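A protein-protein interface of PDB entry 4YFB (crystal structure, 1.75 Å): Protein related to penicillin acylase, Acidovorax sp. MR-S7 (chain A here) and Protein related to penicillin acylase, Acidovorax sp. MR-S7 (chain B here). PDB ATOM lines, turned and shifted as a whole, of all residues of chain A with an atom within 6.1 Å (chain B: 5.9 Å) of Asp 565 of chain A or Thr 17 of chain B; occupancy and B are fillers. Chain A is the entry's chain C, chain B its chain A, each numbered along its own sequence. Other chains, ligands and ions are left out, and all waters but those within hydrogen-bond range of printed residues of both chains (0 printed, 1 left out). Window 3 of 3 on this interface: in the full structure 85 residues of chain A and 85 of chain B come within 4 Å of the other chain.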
ATOM      1  N   HIS A 537      10.751 -14.339 -20.554  1.00  0.00           N
ATOM      2  CA  HIS A 537      10.448 -15.483 -19.643  1.00  0.00           C
ATOM      3  C   HIS A 537      11.627 -16.415 -19.396  1.00  0.00           C
ATOM      4  O   HIS A 537      11.422 -17.554 -18.993  1.00  0.00           O
ATOM      5  CB  HIS A 537       9.196 -16.214 -20.094  1.00  0.00           C
ATOM      6  CG  HIS A 537       8.072 -15.267 -20.412  1.00  0.00           C
ATOM      7  ND1 HIS A 537       7.653 -14.318 -19.522  1.00  0.00           N
ATOM      8  CD2 HIS A 537       7.330 -15.085 -21.567  1.00  0.00           C
ATOM      9  CE1 HIS A 537       6.639 -13.576 -20.086  1.00  0.00           C
ATOM     10  NE2 HIS A 537       6.429 -14.051 -21.318  1.00  0.00           N
ATOM     11  N   ASP A 540      12.317 -14.066 -15.380  1.00  0.00           N
ATOM     12  CA  ASP A 540      11.261 -13.429 -14.543  1.00  0.00           C
ATOM     13  C   ASP A 540      10.799 -14.242 -13.362  1.00  0.00           C
ATOM     14  O   ASP A 540      10.658 -13.741 -12.198  1.00  0.00           O
ATOM     15  CB  ASP A 540      10.082 -12.917 -15.385  1.00  0.00           C
ATOM     16  CG  ASP A 540       9.466 -13.975 -16.320  1.00  0.00           C
ATOM     17  OD1 ASP A 540       9.960 -15.100 -16.395  1.00  0.00           O
ATOM     18  OD2 ASP A 540       8.448 -13.639 -16.992  1.00  0.00           O
ATOM     19  N   TYR A 541      10.564 -15.523 -13.645  1.00  0.00           N
ATOM     20  CA  TYR A 541      10.101 -16.383 -12.558  1.00  0.00           C
ATOM     21  C   TYR A 541      11.241 -16.580 -11.551  1.00  0.00           C
ATOM     22  O   TYR A 541      10.994 -16.784 -10.356  1.00  0.00           O
ATOM     23  CB  TYR A 541       9.705 -17.717 -13.184  1.00  0.00           C
ATOM     24  CG  TYR A 541       8.318 -18.290 -12.767  1.00  0.00           C
ATOM     25  CD1 TYR A 541       7.803 -18.122 -11.464  1.00  0.00           C
ATOM     26  CD2 TYR A 541       7.593 -19.032 -13.701  1.00  0.00           C
ATOM     27  CE1 TYR A 541       6.567 -18.651 -11.080  1.00  0.00           C
ATOM     28  CE2 TYR A 541       6.387 -19.615 -13.336  1.00  0.00           C
ATOM     29  CZ  TYR A 541       5.893 -19.436 -12.030  1.00  0.00           C
ATOM     30  OH  TYR A 541       4.717 -20.106 -11.696  1.00  0.00           O
ATOM     31  N   LEU A 551       3.794 -17.143  -7.081  1.00  0.00           N
ATOM     32  CA  LEU A 551       2.889 -16.616  -8.121  1.00  0.00           C
ATOM     33  C   LEU A 551       1.470 -17.198  -7.874  1.00  0.00           C
ATOM     34  O   LEU A 551       1.271 -18.423  -7.764  1.00  0.00           O
ATOM     35  CB  LEU A 551       3.393 -17.061  -9.510  1.00  0.00           C
ATOM     36  CG  LEU A 551       2.482 -16.510 -10.623  1.00  0.00           C
ATOM     37  CD1 LEU A 551       2.745 -15.015 -10.803  1.00  0.00           C
ATOM     38  CD2 LEU A 551       2.727 -17.328 -11.892  1.00  0.00           C
ATOM     39  N   PRO A 554      -3.424 -17.648 -12.386  1.00  0.00           N
ATOM     40  CA  PRO A 554      -4.881 -17.566 -12.755  1.00  0.00           C
ATOM     41  C   PRO A 554      -5.368 -18.884 -13.318  1.00  0.00           C
ATOM     42  O   PRO A 554      -4.612 -19.600 -13.961  1.00  0.00           O
ATOM     43  CB  PRO A 554      -4.969 -16.467 -13.817  1.00  0.00           C
ATOM     44  CG  PRO A 554      -3.552 -16.074 -14.171  1.00  0.00           C
ATOM     45  CD  PRO A 554      -2.558 -16.742 -13.190  1.00  0.00           C
ATOM     46  N   GLY A 562      -8.444 -11.186 -16.457  1.00  0.00           N
ATOM     47  CA  GLY A 562      -8.206 -10.053 -15.564  1.00  0.00           C
ATOM     48  C   GLY A 562      -6.751  -9.929 -15.140  1.00  0.00           C
ATOM     49  O   GLY A 562      -6.378  -8.926 -14.522  1.00  0.00           O
ATOM     50  N   ASN A 563      -5.908 -10.886 -15.515  1.00  0.00           N
ATOM     51  CA  ASN A 563      -4.486 -10.838 -15.153  1.00  0.00           C
ATOM     52  C   ASN A 563      -3.784  -9.620 -15.762  1.00  0.00           C
ATOM     53  O   ASN A 563      -4.117  -9.213 -16.883  1.00  0.00           O
ATOM     54  CB  ASN A 563      -3.807 -12.152 -15.542  1.00  0.00           C
ATOM     55  CG  ASN A 563      -2.303 -12.116 -15.281  1.00  0.00           C
ATOM     56  OD1 ASN A 563      -1.825 -12.463 -14.128  1.00  0.00           O
ATOM     57  ND2 ASN A 563      -1.542 -11.807 -16.288  1.00  0.00           N
ATOM     58  N   ALA A 564      -2.897  -8.975 -14.976  1.00  0.00           N
ATOM     59  CA  ALA A 564      -2.283  -7.693 -15.385  1.00  0.00           C
ATOM     60  C   ALA A 564      -1.449  -7.841 -16.661  1.00  0.00           C
ATOM     61  O   ALA A 564      -1.230  -6.872 -17.339  1.00  0.00           O
ATOM     62  CB  ALA A 564      -1.390  -7.149 -14.259  1.00  0.00           C
ATOM     63  N   ASP A 565      -0.992  -9.068 -16.977  1.00  0.00           N
ATOM     64  CA  ASP A 565      -0.144  -9.300 -18.141  1.00  0.00           C
ATOM     65  C   ASP A 565      -0.845 -10.054 -19.276  1.00  0.00           C
ATOM     66  O   ASP A 565      -0.206 -10.545 -20.190  1.00  0.00           O
ATOM     67  CB  ASP A 565       1.145 -10.049 -17.731  1.00  0.00           C
ATOM     68  CG  ASP A 565       1.892  -9.271 -16.658  1.00  0.00           C
ATOM     69  OD1 ASP A 565       2.317  -8.152 -16.983  1.00  0.00           O
ATOM     70  OD2 ASP A 565       1.970  -9.715 -15.489  1.00  0.00           O
ATOM     71  N   TYR A 566      -2.167 -10.090 -19.224  1.00  0.00           N
ATOM     72  CA  TYR A 566      -2.889 -10.936 -20.106  1.00  0.00           C
ATOM     73  C   TYR A 566      -2.705 -10.564 -21.574  1.00  0.00           C
ATOM     74  O   TYR A 566      -2.899  -9.414 -21.959  1.00  0.00           O
ATOM     75  CB  TYR A 566      -4.391 -10.757 -19.735  1.00  0.00           C
ATOM     76  CG  TYR A 566      -5.415 -11.346 -20.725  1.00  0.00           C
ATOM     77  CD1 TYR A 566      -5.436 -12.716 -21.043  1.00  0.00           C
ATOM     78  CD2 TYR A 566      -6.332 -10.491 -21.388  1.00  0.00           C
ATOM     79  CE1 TYR A 566      -6.414 -13.237 -21.938  1.00  0.00           C
ATOM     80  CE2 TYR A 566      -7.267 -10.983 -22.297  1.00  0.00           C
ATOM     81  CZ  TYR A 566      -7.288 -12.359 -22.566  1.00  0.00           C
ATOM     82  OH  TYR A 566      -8.207 -12.951 -23.426  1.00  0.00           O
ATOM     83  N   ARG A 567      -2.409 -11.562 -22.395  1.00  0.00           N
ATOM     84  CA  ARG A 567      -2.416 -11.362 -23.844  1.00  0.00           C
ATOM     85  C   ARG A 567      -3.088 -12.570 -24.420  1.00  0.00           C
ATOM     86  O   ARG A 567      -2.970 -13.660 -23.820  1.00  0.00           O
ATOM     87  CB  ARG A 567      -0.974 -11.350 -24.350  1.00  0.00           C
ATOM     88  CG  ARG A 567      -0.176 -10.142 -23.837  1.00  0.00           C
ATOM     89  CD  ARG A 567      -0.105  -9.331 -25.057  1.00  0.00           C
ATOM     90  NE  ARG A 567       0.190  -7.931 -24.781  1.00  0.00           N
ATOM     91  CZ  ARG A 567      -0.708  -7.036 -24.389  1.00  0.00           C
ATOM     92  NH1 ARG A 567      -0.301  -5.759 -24.282  1.00  0.00           N
ATOM     93  NH2 ARG A 567      -1.997  -7.421 -24.147  1.00  0.00           N
ATOM     94  N   ARG B  15      -1.671 -15.761 -22.457  1.00  0.00           N
ATOM     95  CA  ARG B  15      -0.522 -15.847 -21.559  1.00  0.00           C
ATOM     96  C   ARG B  15      -0.740 -14.868 -20.456  1.00  0.00           C
ATOM     97  O   ARG B  15      -1.301 -13.790 -20.671  1.00  0.00           O
ATOM     98  CB  ARG B  15       0.754 -15.529 -22.321  1.00  0.00           C
ATOM     99  CG  ARG B  15       1.208 -16.793 -23.035  1.00  0.00           C
ATOM    100  CD  ARG B  15       2.571 -16.562 -23.660  1.00  0.00           C
ATOM    101  NE  ARG B  15       3.034 -17.570 -24.622  1.00  0.00           N
ATOM    102  CZ  ARG B  15       3.957 -18.515 -24.341  1.00  0.00           C
ATOM    103  NH1 ARG B  15       4.433 -19.281 -25.313  1.00  0.00           N
ATOM    104  NH2 ARG B  15       4.367 -18.718 -23.088  1.00  0.00           N
ATOM    105  N   THR B  16      -0.291 -15.251 -19.257  1.00  0.00           N
ATOM    106  CA  THR B  16      -0.386 -14.352 -18.087  1.00  0.00           C
ATOM    107  C   THR B  16       1.033 -14.124 -17.510  1.00  0.00           C
ATOM    108  O   THR B  16       2.067 -14.444 -18.167  1.00  0.00           O
ATOM    109  CB  THR B  16      -1.355 -14.904 -17.048  1.00  0.00           C
ATOM    110  OG1 THR B  16      -0.931 -16.242 -16.651  1.00  0.00           O
ATOM    111  CG2 THR B  16      -2.753 -14.965 -17.722  1.00  0.00           C
ATOM    112  N   THR B  17       1.064 -13.584 -16.307  1.00  0.00           N
ATOM    113  CA  THR B  17       2.346 -13.257 -15.624  1.00  0.00           C
ATOM    114  C   THR B  17       3.295 -14.454 -15.673  1.00  0.00           C
ATOM    115  O   THR B  17       2.863 -15.608 -15.474  1.00  0.00           O
ATOM    116  CB  THR B  17       2.039 -12.832 -14.161  1.00  0.00           C
ATOM    117  OG1 THR B  17       1.023 -11.823 -14.209  1.00  0.00           O
ATOM    118  CG2 THR B  17       3.262 -12.230 -13.452  1.00  0.00           C
ATOM    119  N   MET B  18       4.573 -14.131 -15.911  1.00  0.00           N
ATOM    120  CA  MET B  18       5.653 -15.124 -16.140  1.00  0.00           C
ATOM    121  C   MET B  18       5.504 -15.895 -17.432  1.00  0.00           C
ATOM    122  O   MET B  18       6.279 -16.840 -17.676  1.00  0.00           O
ATOM    123  CB  MET B  18       5.768 -16.120 -14.959  1.00  0.00           C
ATOM    124  CG  MET B  18       5.795 -15.505 -13.590  1.00  0.00           C
ATOM    125  SD  MET B  18       7.114 -14.275 -13.416  1.00  0.00           S
ATOM    126  CE  MET B  18       6.870 -13.737 -11.705  1.00  0.00           C
ATOM    127  N   GLY B  19       4.581 -15.451 -18.304  1.00  0.00           N
ATOM    128  CA  GLY B  19       4.382 -16.091 -19.594  1.00  0.00           C
ATOM    129  C   GLY B  19       3.555 -17.402 -19.544  1.00  0.00           C
ATOM    130  O   GLY B  19       3.344 -17.993 -20.607  1.00  0.00           O
ATOM    131  N   VAL B  20       3.011 -17.769 -18.381  1.00  0.00           N
ATOM    132  CA  VAL B  20       2.292 -19.080 -18.285  1.00  0.00           C
ATOM    133  C   VAL B  20       1.196 -19.073 -19.336  1.00  0.00           C
ATOM    134  O   VAL B  20       0.398 -18.121 -19.349  1.00  0.00           O
ATOM    135  CB  VAL B  20       1.665 -19.218 -16.913  1.00  0.00           C
ATOM    136  CG1 VAL B  20       0.785 -20.494 -16.876  1.00  0.00           C
ATOM    137  CG2 VAL B  20       2.804 -19.307 -15.892  1.00  0.00           C
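CG2 of Thr 17 of chain B touches CD1 of Leu 551 of chain A (3.9 Å). Met 18 of chain B touches Leu 551 of chain A (CG to CD2, 3.95 Å). Pro 554 of chain A touches Thr 16 of chain B (CG to OG1, 3.6 Å). Thr 16 of chain B touches Asn 563 of chain A. Arg 15 of chain B touches Tyr 566 of chain A (O to CA, 3.3 Å).
Printed residues of chain B within 4 Å of His 537 of chain A: Met 18 and Gly 19. Of the printed residues of chain B, Asp 540 of chain A touches Met 18. Of the printed residues of chain B, Tyr 541 of chain A touches Met 18 (3.7 Å). Of the printed residues of chain B, Leu 551 of chain A touches Thr 17 (3.9 Å) and Met 18 (3.95 Å). Ala 564 of chain A touches none of the printed residues of chain B. Asp 565 of chain A touches two residues of chain B. Val 20 of chain B touches none of the printed residues of chain A. The nearest residue of chain A that does not touch Thr 17 of chain B is Ala 564 of chain A (4.9 Å).
Hydrophobic or aromatic side chains of chain A that line the printed part of chain B: His 537, Tyr 541, Leu 551 and Pro 554. Among the printed residues, 13 pairs touch across the chains. Among the printed residues, no Asp or Glu carboxylate lies within 4 Å of a Lys or Arg side-chain nitrogen of the other chain.
The guanidinium group (NH2) of Arg 15 of chain B sits at hydrogen-bond distance from the backbone carbonyl oxygen (O) of Gly 19 of chain B (2.8 Å). OD2 of Asp 540 of chain A lies within hydrogen-bond range of ND1 of His 537 of chain A (2.7 Å). The side-chain amide nitrogen (ND2) of Asn 563 of chain A lies close to the backbone NH (N) of Asp 565 of chain A, at 2.9 Å. The backbone NH of Tyr 566 of chain A lies close to the side-chain amide nitrogen of Asn 563 of chain A, at 3.5 Å.
O of Arg 567 of chain A is in hydrogen-bond range of N of Arg 15 of chain B. OG1 of Thr 17 of chain B sits at hydrogen-bond distance from OD1 of Asn 563 of chain A, at 2.9 Å. OG1 of Thr 17 of chain B is in hydrogen-bond range of OD2 of Asp 565 of chain A. A ring nitrogen (ND1) of His 537 of chain A lies close to the backbone carbonyl oxygen (O) of Met 18 of chain B (3.4 Å). SD of Met 18 of chain B lies within hydrogen-bond range of N of Tyr 541 of chain A, 3.7 Å away. The backbone NH (N) of Gly 19 of chain B lies close to a ring nitrogen (ND1) of His 537 of chain A. The backbone carbonyl oxygen (O) of Asp 540 of chain A sits close to the side-chain sulfur (SD) of Met 18 of chain B (3.8 Å). The backbone carbonyl oxygen of Asp 565 of chain A sits close to the backbone carbonyl oxygen of Arg 15 of chain B, 3.5 Å away.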
